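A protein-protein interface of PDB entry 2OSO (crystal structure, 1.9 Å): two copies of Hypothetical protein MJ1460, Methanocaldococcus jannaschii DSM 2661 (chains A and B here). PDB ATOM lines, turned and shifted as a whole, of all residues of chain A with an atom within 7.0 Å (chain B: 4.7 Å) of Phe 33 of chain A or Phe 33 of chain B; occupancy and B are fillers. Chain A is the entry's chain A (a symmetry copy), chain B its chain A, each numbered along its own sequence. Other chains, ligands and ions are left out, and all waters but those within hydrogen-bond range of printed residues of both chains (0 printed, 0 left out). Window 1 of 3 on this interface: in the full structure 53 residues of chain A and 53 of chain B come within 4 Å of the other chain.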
ATOM      1  N   ILE A  12      15.429   5.913  -7.049  1.00  0.00           N
ATOM      2  CA  ILE A  12      14.465   6.580  -6.166  1.00  0.00           C
ATOM      3  C   ILE A  12      14.446   5.946  -4.765  1.00  0.00           C
ATOM      4  O   ILE A  12      14.396   6.668  -3.772  1.00  0.00           O
ATOM      5  CB  ILE A  12      13.034   6.649  -6.791  1.00  0.00           C
ATOM      6  CG1 ILE A  12      12.993   7.677  -7.934  1.00  0.00           C
ATOM      7  CG2 ILE A  12      11.995   7.034  -5.745  1.00  0.00           C
ATOM      8  CD1 ILE A  12      12.348   7.127  -9.184  1.00  0.00           C
ATOM      9  N   ILE A  28       8.873  19.972  -7.324  1.00  0.00           N
ATOM     10  CA  ILE A  28       7.746  20.079  -8.248  1.00  0.00           C
ATOM     11  C   ILE A  28       6.525  20.649  -7.545  1.00  0.00           C
ATOM     12  O   ILE A  28       6.172  20.171  -6.457  1.00  0.00           O
ATOM     13  CB  ILE A  28       7.437  18.712  -8.896  1.00  0.00           C
ATOM     14  CG1 ILE A  28       6.609  18.877 -10.157  1.00  0.00           C
ATOM     15  CG2 ILE A  28       6.709  17.740  -7.947  1.00  0.00           C
ATOM     16  CD1 ILE A  28       6.409  17.546 -10.911  1.00  0.00           C
ATOM     17  N   PRO A  29       5.908  21.696  -8.125  1.00  0.00           N
ATOM     18  CA  PRO A  29       4.601  22.206  -7.636  1.00  0.00           C
ATOM     19  C   PRO A  29       3.494  21.125  -7.538  1.00  0.00           C
ATOM     20  O   PRO A  29       3.262  20.361  -8.505  1.00  0.00           O
ATOM     21  CB  PRO A  29       4.214  23.227  -8.684  1.00  0.00           C
ATOM     22  CG  PRO A  29       5.468  23.650  -9.322  1.00  0.00           C
ATOM     23  CD  PRO A  29       6.375  22.467  -9.302  1.00  0.00           C
ATOM     24  N   MET A  30       2.852  21.058  -6.370  1.00  0.00           N
ATOM     25  CA  MET A  30       1.787  20.078  -6.048  1.00  0.00           C
ATOM     26  C   MET A  30       0.730  19.827  -7.139  1.00  0.00           C
ATOM     27  O   MET A  30       0.337  18.687  -7.349  1.00  0.00           O
ATOM     28  CB  MET A  30       1.083  20.467  -4.729  1.00  0.00           C
ATOM     29  CG  MET A  30       0.218  19.369  -4.108  1.00  0.00           C
ATOM     30  SD  MET A  30       1.323  17.972  -3.305  1.00  0.00           S
ATOM     31  CE  MET A  30       0.070  16.491  -3.201  1.00  0.00           C
ATOM     32  N   PRO A  31       0.266  20.872  -7.836  1.00  0.00           N
ATOM     33  CA  PRO A  31      -0.725  20.614  -8.939  1.00  0.00           C
ATOM     34  C   PRO A  31      -0.257  19.577  -9.999  1.00  0.00           C
ATOM     35  O   PRO A  31      -1.090  18.805 -10.508  1.00  0.00           O
ATOM     36  CB  PRO A  31      -0.951  22.003  -9.535  1.00  0.00           C
ATOM     37  CG  PRO A  31      -0.653  22.947  -8.386  1.00  0.00           C
ATOM     38  CD  PRO A  31       0.548  22.316  -7.716  1.00  0.00           C
ATOM     39  N   TYR A  32       1.046  19.518 -10.267  1.00  0.00           N
ATOM     40  CA  TYR A  32       1.597  18.599 -11.238  1.00  0.00           C
ATOM     41  C   TYR A  32       1.778  17.181 -10.688  1.00  0.00           C
ATOM     42  O   TYR A  32       1.672  16.195 -11.416  1.00  0.00           O
ATOM     43  CB  TYR A  32       2.939  19.140 -11.734  1.00  0.00           C
ATOM     44  CG  TYR A  32       2.799  20.423 -12.529  1.00  0.00           C
ATOM     45  CD1 TYR A  32       2.111  20.438 -13.750  1.00  0.00           C
ATOM     46  CD2 TYR A  32       3.395  21.606 -12.094  1.00  0.00           C
ATOM     47  CE1 TYR A  32       2.013  21.574 -14.493  1.00  0.00           C
ATOM     48  CE2 TYR A  32       3.284  22.762 -12.846  1.00  0.00           C
ATOM     49  CZ  TYR A  32       2.584  22.743 -14.022  1.00  0.00           C
ATOM     50  OH  TYR A  32       2.469  23.860 -14.785  1.00  0.00           O
ATOM     51  N   PHE A  33       2.048  17.100  -9.393  1.00  0.00           N
ATOM     52  CA  PHE A  33       2.069  15.851  -8.665  1.00  0.00           C
ATOM     53  C   PHE A  33       0.644  15.267  -8.701  1.00  0.00           C
ATOM     54  O   PHE A  33       0.453  14.141  -9.034  1.00  0.00           O
ATOM     55  CB  PHE A  33       2.562  16.099  -7.234  1.00  0.00           C
ATOM     56  CG  PHE A  33       2.615  14.865  -6.372  1.00  0.00           C
ATOM     57  CD1 PHE A  33       1.483  14.397  -5.729  1.00  0.00           C
ATOM     58  CD2 PHE A  33       3.803  14.225  -6.147  1.00  0.00           C
ATOM     59  CE1 PHE A  33       1.544  13.274  -4.924  1.00  0.00           C
ATOM     60  CE2 PHE A  33       3.854  13.081  -5.325  1.00  0.00           C
ATOM     61  CZ  PHE A  33       2.735  12.614  -4.746  1.00  0.00           C
ATOM     62  N   GLY A  34      -0.385  16.064  -8.444  1.00  0.00           N
ATOM     63  CA  GLY A  34      -1.705  15.564  -8.569  1.00  0.00           C
ATOM     64  C   GLY A  34      -2.157  15.186  -9.943  1.00  0.00           C
ATOM     65  O   GLY A  34      -2.935  14.256 -10.097  1.00  0.00           O
ATOM     66  N   LEU A  35      -1.716  15.926 -10.940  1.00  0.00           N
ATOM     67  CA  LEU A  35      -2.035  15.638 -12.341  1.00  0.00           C
ATOM     68  C   LEU A  35      -1.519  14.282 -12.756  1.00  0.00           C
ATOM     69  O   LEU A  35      -2.166  13.558 -13.503  1.00  0.00           O
ATOM     70  CB  LEU A  35      -1.456  16.738 -13.262  1.00  0.00           C
ATOM     71  CG  LEU A  35      -1.813  16.523 -14.749  1.00  0.00           C
ATOM     72  CD1 LEU A  35      -3.300  16.521 -14.974  1.00  0.00           C
ATOM     73  CD2 LEU A  35      -1.148  17.477 -15.714  1.00  0.00           C
ATOM     74  N   PHE A  36      -0.350  13.926 -12.255  1.00  0.00           N
ATOM     75  CA  PHE A  36       0.214  12.602 -12.486  1.00  0.00           C
ATOM     76  C   PHE A  36      -0.740  11.479 -12.043  1.00  0.00           C
ATOM     77  O   PHE A  36      -0.994  10.511 -12.781  1.00  0.00           O
ATOM     78  CB  PHE A  36       1.547  12.505 -11.780  1.00  0.00           C
ATOM     79  CG  PHE A  36       2.324  11.265 -12.136  1.00  0.00           C
ATOM     80  CD1 PHE A  36       3.096  11.248 -13.274  1.00  0.00           C
ATOM     81  CD2 PHE A  36       2.266  10.137 -11.336  1.00  0.00           C
ATOM     82  CE1 PHE A  36       3.814  10.121 -13.638  1.00  0.00           C
ATOM     83  CE2 PHE A  36       2.975   8.973 -11.691  1.00  0.00           C
ATOM     84  CZ  PHE A  36       3.769   8.988 -12.840  1.00  0.00           C
ATOM     85  N   ALA A  37      -1.258  11.614 -10.830  1.00  0.00           N
ATOM     86  CA  ALA A  37      -2.110  10.648 -10.264  1.00  0.00           C
ATOM     87  C   ALA A  37      -3.402  10.608 -11.099  1.00  0.00           C
ATOM     88  O   ALA A  37      -3.970   9.560 -11.342  1.00  0.00           O
ATOM     89  CB  ALA A  37      -2.408  11.013  -8.769  1.00  0.00           C
ATOM     90  N   LEU A  38      -3.885  11.774 -11.505  1.00  0.00           N
ATOM     91  CA  LEU A  38      -5.114  11.866 -12.297  1.00  0.00           C
ATOM     92  C   LEU A  38      -4.925  11.130 -13.627  1.00  0.00           C
ATOM     93  O   LEU A  38      -5.836  10.423 -14.108  1.00  0.00           O
ATOM     94  CB  LEU A  38      -5.461  13.339 -12.564  1.00  0.00           C
ATOM     95  CG  LEU A  38      -6.703  13.665 -13.398  1.00  0.00           C
ATOM     96  CD1 LEU A  38      -7.113  15.117 -13.100  1.00  0.00           C
ATOM     97  CD2 LEU A  38      -6.471  13.451 -14.897  1.00  0.00           C
ATOM     98  N   LEU A  53      -6.624   6.746  -3.852  1.00  0.00           N
ATOM     99  CA  LEU A  53      -5.520   7.521  -3.293  1.00  0.00           C
ATOM    100  C   LEU A  53      -5.159   7.103  -1.835  1.00  0.00           C
ATOM    101  O   LEU A  53      -3.997   7.146  -1.440  1.00  0.00           O
ATOM    102  CB  LEU A  53      -5.832   9.013  -3.381  1.00  0.00           C
ATOM    103  CG  LEU A  53      -5.594   9.557  -4.813  1.00  0.00           C
ATOM    104  CD1 LEU A  53      -6.048  10.947  -4.921  1.00  0.00           C
ATOM    105  CD2 LEU A  53      -4.091   9.483  -5.147  1.00  0.00           C
ATOM    106  N   PHE A  60       2.613   3.698  -0.010  1.00  0.00           N
ATOM    107  CA  PHE A  60       3.621   4.754   0.028  1.00  0.00           C
ATOM    108  C   PHE A  60       4.232   4.831   1.425  1.00  0.00           C
ATOM    109  O   PHE A  60       5.458   4.745   1.567  1.00  0.00           O
ATOM    110  CB  PHE A  60       2.963   6.054  -0.390  1.00  0.00           C
ATOM    111  CG  PHE A  60       3.908   7.145  -0.776  1.00  0.00           C
ATOM    112  CD1 PHE A  60       4.416   7.981   0.183  1.00  0.00           C
ATOM    113  CD2 PHE A  60       4.207   7.385  -2.134  1.00  0.00           C
ATOM    114  CE1 PHE A  60       5.237   9.054  -0.168  1.00  0.00           C
ATOM    115  CE2 PHE A  60       5.008   8.399  -2.495  1.00  0.00           C
ATOM    116  CZ  PHE A  60       5.545   9.255  -1.523  1.00  0.00           C
ATOM    117  N   MET A  79       9.006  16.139   2.748  1.00  0.00           N
ATOM    118  CA  MET A  79       8.070  16.081   1.643  1.00  0.00           C
ATOM    119  C   MET A  79       7.399  17.444   1.390  1.00  0.00           C
ATOM    120  O   MET A  79       6.788  17.652   0.338  1.00  0.00           O
ATOM    121  CB  MET A  79       7.019  15.030   1.941  1.00  0.00           C
ATOM    122  CG  MET A  79       7.469  13.625   1.985  1.00  0.00           C
ATOM    123  SD  MET A  79       5.908  12.393   2.161  1.00  0.00           S
ATOM    124  CE  MET A  79       5.285  12.432   0.326  1.00  0.00           C
ATOM    125  N   PHE A  81       4.978  18.428   3.205  1.00  0.00           N
ATOM    126  CA  PHE A  81       3.555  18.095   3.444  1.00  0.00           C
ATOM    127  C   PHE A  81       3.001  18.729   4.729  1.00  0.00           C
ATOM    128  O   PHE A  81       1.820  18.616   5.010  1.00  0.00           O
ATOM    129  CB  PHE A  81       3.401  16.548   3.450  1.00  0.00           C
ATOM    130  CG  PHE A  81       3.038  15.959   2.106  1.00  0.00           C
ATOM    131  CD1 PHE A  81       3.404  16.580   0.925  1.00  0.00           C
ATOM    132  CD2 PHE A  81       2.353  14.761   2.046  1.00  0.00           C
ATOM    133  CE1 PHE A  81       3.033  16.068  -0.284  1.00  0.00           C
ATOM    134  CE2 PHE A  81       1.974  14.219   0.871  1.00  0.00           C
ATOM    135  CZ  PHE A  81       2.315  14.868  -0.338  1.00  0.00           C
ATOM    136  N   TYR A 107      -2.510  21.856  -0.795  1.00  0.00           N
ATOM    137  CA  TYR A 107      -3.819  22.122  -1.344  1.00  0.00           C
ATOM    138  C   TYR A 107      -4.631  23.120  -0.539  1.00  0.00           C
ATOM    139  O   TYR A 107      -5.823  22.962  -0.467  1.00  0.00           O
ATOM    140  CB  TYR A 107      -4.640  20.839  -1.456  1.00  0.00           C
ATOM    141  CG  TYR A 107      -4.021  19.815  -2.345  1.00  0.00           C
ATOM    142  CD1 TYR A 107      -3.745  20.122  -3.668  1.00  0.00           C
ATOM    143  CD2 TYR A 107      -3.773  18.534  -1.900  1.00  0.00           C
ATOM    144  CE1 TYR A 107      -3.203  19.208  -4.505  1.00  0.00           C
ATOM    145  CE2 TYR A 107      -3.233  17.579  -2.742  1.00  0.00           C
ATOM    146  CZ  TYR A 107      -2.953  17.938  -4.063  1.00  0.00           C
ATOM    147  OH  TYR A 107      -2.382  17.055  -4.967  1.00  0.00           O
ATOM    148  N   PHE A 119      -4.868  10.746   0.328  1.00  0.00           N
ATOM    149  CA  PHE A 119      -3.476  10.241   0.149  1.00  0.00           C
ATOM    150  C   PHE A 119      -2.675  10.359   1.448  1.00  0.00           C
ATOM    151  O   PHE A 119      -2.087   9.375   1.907  1.00  0.00           O
ATOM    152  CB  PHE A 119      -2.793  10.953  -1.038  1.00  0.00           C
ATOM    153  CG  PHE A 119      -1.375  10.557  -1.261  1.00  0.00           C
ATOM    154  CD1 PHE A 119      -1.060   9.243  -1.595  1.00  0.00           C
ATOM    155  CD2 PHE A 119      -0.359  11.492  -1.242  1.00  0.00           C
ATOM    156  CE1 PHE A 119       0.263   8.878  -1.787  1.00  0.00           C
ATOM    157  CE2 PHE A 119       0.955  11.100  -1.477  1.00  0.00           C
ATOM    158  CZ  PHE A 119       1.238   9.795  -1.782  1.00  0.00           C
ATOM    159  N   ILE B  28       7.040  19.757  -3.967  1.00  0.00           N
ATOM    160  CA  ILE B  28       7.471  18.442  -3.501  1.00  0.00           C
ATOM    161  C   ILE B  28       8.796  18.053  -4.135  1.00  0.00           C
ATOM    162  O   ILE B  28       8.939  18.165  -5.362  1.00  0.00           O
ATOM    163  CB  ILE B  28       6.383  17.380  -3.772  1.00  0.00           C
ATOM    164  CG1 ILE B  28       6.596  16.145  -2.915  1.00  0.00           C
ATOM    165  CG2 ILE B  28       6.306  16.952  -5.250  1.00  0.00           C
ATOM    166  CD1 ILE B  28       5.444  15.127  -3.049  1.00  0.00           C
ATOM    167  N   PRO B  29       9.782  17.647  -3.313  1.00  0.00           N
ATOM    168  CA  PRO B  29      11.045  17.060  -3.831  1.00  0.00           C
ATOM    169  C   PRO B  29      10.840  15.861  -4.792  1.00  0.00           C
ATOM    170  O   PRO B  29      10.087  14.911  -4.473  1.00  0.00           O
ATOM    171  CB  PRO B  29      11.747  16.584  -2.576  1.00  0.00           C
ATOM    172  CG  PRO B  29      11.196  17.387  -1.476  1.00  0.00           C
ATOM    173  CD  PRO B  29       9.779  17.683  -1.831  1.00  0.00           C
ATOM    174  N   MET B  30      11.487  15.936  -5.956  1.00  0.00           N
ATOM    175  CA  MET B  30      11.404  14.920  -7.033  1.00  0.00           C
ATOM    176  C   MET B  30      11.468  13.444  -6.595  1.00  0.00           C
ATOM    177  O   MET B  30      10.733  12.624  -7.126  1.00  0.00           O
ATOM    178  CB  MET B  30      12.484  15.186  -8.104  1.00  0.00           C
ATOM    179  CG  MET B  30      12.288  14.438  -9.424  1.00  0.00           C
ATOM    180  SD  MET B  30      10.824  15.213 -10.461  1.00  0.00           S
ATOM    181  CE  MET B  30      10.391  13.759 -11.676  1.00  0.00           C
ATOM    182  N   PRO B  31      12.333  13.098  -5.634  1.00  0.00           N
ATOM    183  CA  PRO B  31      12.352  11.667  -5.169  1.00  0.00           C
ATOM    184  C   PRO B  31      10.973  11.118  -4.710  1.00  0.00           C
ATOM    185  O   PRO B  31      10.679   9.931  -4.941  1.00  0.00           O
ATOM    186  CB  PRO B  31      13.385  11.680  -4.043  1.00  0.00           C
ATOM    187  CG  PRO B  31      14.297  12.840  -4.397  1.00  0.00           C
ATOM    188  CD  PRO B  31      13.340  13.895  -4.906  1.00  0.00           C
ATOM    189  N   TYR B  32      10.130  11.976  -4.140  1.00  0.00           N
ATOM    190  CA  TYR B  32       8.823  11.580  -3.665  1.00  0.00           C
ATOM    191  C   TYR B  32       7.778  11.496  -4.784  1.00  0.00           C
ATOM    192  O   TYR B  32       6.852  10.688  -4.734  1.00  0.00           O
ATOM    193  CB  TYR B  32       8.359  12.566  -2.592  1.00  0.00           C
ATOM    194  CG  TYR B  32       9.201  12.507  -1.334  1.00  0.00           C
ATOM    195  CD1 TYR B  32       9.232  11.348  -0.546  1.00  0.00           C
ATOM    196  CD2 TYR B  32       9.925  13.618  -0.902  1.00  0.00           C
ATOM    197  CE1 TYR B  32       9.953  11.295   0.607  1.00  0.00           C
ATOM    198  CE2 TYR B  32      10.667  13.556   0.265  1.00  0.00           C
ATOM    199  CZ  TYR B  32      10.691  12.400   0.996  1.00  0.00           C
ATOM    200  OH  TYR B  32      11.401  12.318   2.150  1.00  0.00           O
ATOM    201  N   PHE B  33       7.947  12.342  -5.789  1.00  0.00           N
ATOM    202  CA  PHE B  33       7.176  12.288  -7.010  1.00  0.00           C
ATOM    203  C   PHE B  33       7.496  10.948  -7.701  1.00  0.00           C
ATOM    204  O   PHE B  33       6.623  10.227  -8.068  1.00  0.00           O
ATOM    205  CB  PHE B  33       7.521  13.495  -7.890  1.00  0.00           C
ATOM    206  CG  PHE B  33       6.783  13.538  -9.203  1.00  0.00           C
ATOM    207  CD1 PHE B  33       7.231  12.818 -10.295  1.00  0.00           C
ATOM    208  CD2 PHE B  33       5.695  14.353  -9.362  1.00  0.00           C
ATOM    209  CE1 PHE B  33       6.559  12.878 -11.503  1.00  0.00           C
ATOM    210  CE2 PHE B  33       5.016  14.406 -10.597  1.00  0.00           C
ATOM    211  CZ  PHE B  33       5.439  13.662 -11.634  1.00  0.00           C
ATOM    212  N   GLY B  34       8.760  10.561  -7.803  1.00  0.00           N
ATOM    213  CA  GLY B  34       9.060   9.289  -8.349  1.00  0.00           C
ATOM    214  C   GLY B  34       8.610   8.095  -7.569  1.00  0.00           C
ATOM    215  O   GLY B  34       8.267   7.077  -8.152  1.00  0.00           O
ATOM    216  N   LEU B  35       8.649   8.192  -6.256  1.00  0.00           N
ATOM    217  CA  LEU B  35       8.187   7.122  -5.369  1.00  0.00           C
ATOM    218  C   LEU B  35       6.722   6.828  -5.577  1.00  0.00           C
ATOM    219  O   LEU B  35       6.292   5.681  -5.538  1.00  0.00           O
ATOM    220  CB  LEU B  35       8.454   7.493  -3.890  1.00  0.00           C
ATOM    221  CG  LEU B  35       8.044   6.376  -2.908  1.00  0.00           C
ATOM    222  CD1 LEU B  35       8.796   5.099  -3.167  1.00  0.00           C
ATOM    223  CD2 LEU B  35       8.137   6.740  -1.444  1.00  0.00           C
ATOM    224  N   PHE B  36       5.948   7.871  -5.819  1.00  0.00           N
ATOM    225  CA  PHE B  36       4.535   7.719  -6.146  1.00  0.00           C
ATOM    226  C   PHE B  36       4.315   6.801  -7.361  1.00  0.00           C
ATOM    227  O   PHE B  36       3.482   5.878  -7.338  1.00  0.00           O
ATOM    228  CB  PHE B  36       3.933   9.087  -6.371  1.00  0.00           C
ATOM    229  CG  PHE B  36       2.432   9.069  -6.491  1.00  0.00           C
ATOM    230  CD1 PHE B  36       1.658   9.081  -5.355  1.00  0.00           C
ATOM    231  CD2 PHE B  36       1.820   9.031  -7.732  1.00  0.00           C
ATOM    232  CE1 PHE B  36       0.274   9.052  -5.428  1.00  0.00           C
ATOM    233  CE2 PHE B  36       0.416   8.986  -7.834  1.00  0.00           C
ATOM    234  CZ  PHE B  36      -0.349   9.021  -6.666  1.00  0.00           C
ATOM    235  N   ALA B  37       5.064   7.067  -8.421  1.00  0.00           N
ATOM    236  CA  ALA B  37       4.946   6.348  -9.625  1.00  0.00           C
ATOM    237  C   ALA B  37       5.381   4.896  -9.355  1.00  0.00           C
ATOM    238  O   ALA B  37       4.804   3.955  -9.864  1.00  0.00           O
ATOM    239  CB  ALA B  37       5.837   7.013 -10.731  1.00  0.00           C
ATOM    240  N   PHE B 119       9.670   9.666 -18.925  1.00  0.00           N
ATOM    241  CA  PHE B 119       8.455  10.480 -18.630  1.00  0.00           C
ATOM    242  C   PHE B 119       8.489  11.815 -19.380  1.00  0.00           C
ATOM    243  O   PHE B 119       7.533  12.157 -20.080  1.00  0.00           O
ATOM    244  CB  PHE B 119       8.285  10.659 -17.106  1.00  0.00           C
ATOM    245  CG  PHE B 119       7.127  11.508 -16.711  1.00  0.00           C
ATOM    246  CD1 PHE B 119       5.831  11.114 -17.023  1.00  0.00           C
ATOM    247  CD2 PHE B 119       7.304  12.646 -15.946  1.00  0.00           C
ATOM    248  CE1 PHE B 119       4.759  11.919 -16.666  1.00  0.00           C
ATOM    249  CE2 PHE B 119       6.204  13.411 -15.570  1.00  0.00           C
ATOM    250  CZ  PHE B 119       4.939  13.009 -15.910  1.00  0.00           C
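O of Ile 28 of chain B lies within hydrogen-bond range of N of Ile 28 of chain A, at 2.7 Å.
Ile 12 of chain A touches Pro 31 of chain B (CG2 to O, 3.3 Å). Gly 34 of chain B touches Ile 12 of chain A (C to CG2, 3.99 Å). Ile 12 of chain A touches Leu 35 of chain B. Ile 28 of chain A touches Phe 33 of chain B. O of Tyr 32 of chain A touches CE2 of Phe 33 of chain B, at 3.9 Å. Phe 36 of chain B touches Phe 33 of chain A. CZ of Phe 33 of chain B touches CD1 of Phe 36 of chain A, at 3.7 Å. CD2 of Phe 36 of chain A touches CD2 of Phe 36 of chain B, at 3.8 Å. Phe 36 of chain A touches Ala 37 of chain B (CZ to CB, 3.6 Å). Met 79 of chain A touches Tyr 32 of chain B.
Phe 33 of chain A touches just these residues of chain B: Ile 28 (3.4 Å), Tyr 32 (3.9 Å), Phe 33 (3.7 Å) and Phe 36 (3.7 Å). Of chain A, only Ile 28 (3.4 Å), Tyr 32 (3.9 Å), Phe 33 (3.7 Å) and Phe 36 (3.7 Å) come within 4 Å of Phe 33 of chain B. Printed residues of chain A within 4 Å of Ala 37 of chain B: Phe 36. Printed residues of chain B within 4 Å of Ala 37 of chain A: Phe 36 (3.6 Å). Of the printed residues of chain A, Ile 28 of chain B touches Ile 28, Phe 33, Met 79 and Phe 81. The nearest printed residue of chain B that does not touch Phe 33 of chain A is Gly 34 of chain B (6.0 Å). The nearest residue of chain A that does not touch Phe 33 of chain B is Phe 60 of chain A (5.8 Å). The nearest printed residue of chain A that does not touch Phe 119 of chain B is Ile 28 of chain A (6.2 Å).
Printed residues of chain A that touch a printed residue of chain B: Ile 12, Ile 28, Tyr 32, Phe 33, Phe 36, Ala 37, Phe 60, Met 79, Phe 81 and Phe 119. Hydrophobic or aromatic side chains of chain A that line the printed part of chain B: Ile 12, Ile 28, Phe 33, Phe 36, Ala 37, Phe 60, Met 79, Phe 81 and Phe 119. Hydrophobic or aromatic side chains of chain B within 4 Å of the printed part of chain A: Ile 28, Pro 29, Tyr 32, Phe 33, Leu 35, Phe 36, Ala 37 and Phe 119. Among the printed residues, 23 pairs touch across the chains.
Ile 28 of chain A touches its own counterpart, Ile 28 of chain B. Tyr 32 of chain A touches Phe 33 of chain B, and with the chains exchanged Phe 33 of chain A touches Tyr 32 of chain B. Phe 33 of chain A touches Phe 36 of chain B, and with the chains exchanged Phe 36 of chain A touches Phe 33 of chain B. Phe 36 of chain A touches Phe 119 of chain B, and with the chains exchanged Phe 119 of chain A touches Phe 36 of chain B. 11 positions are printed for both chains.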
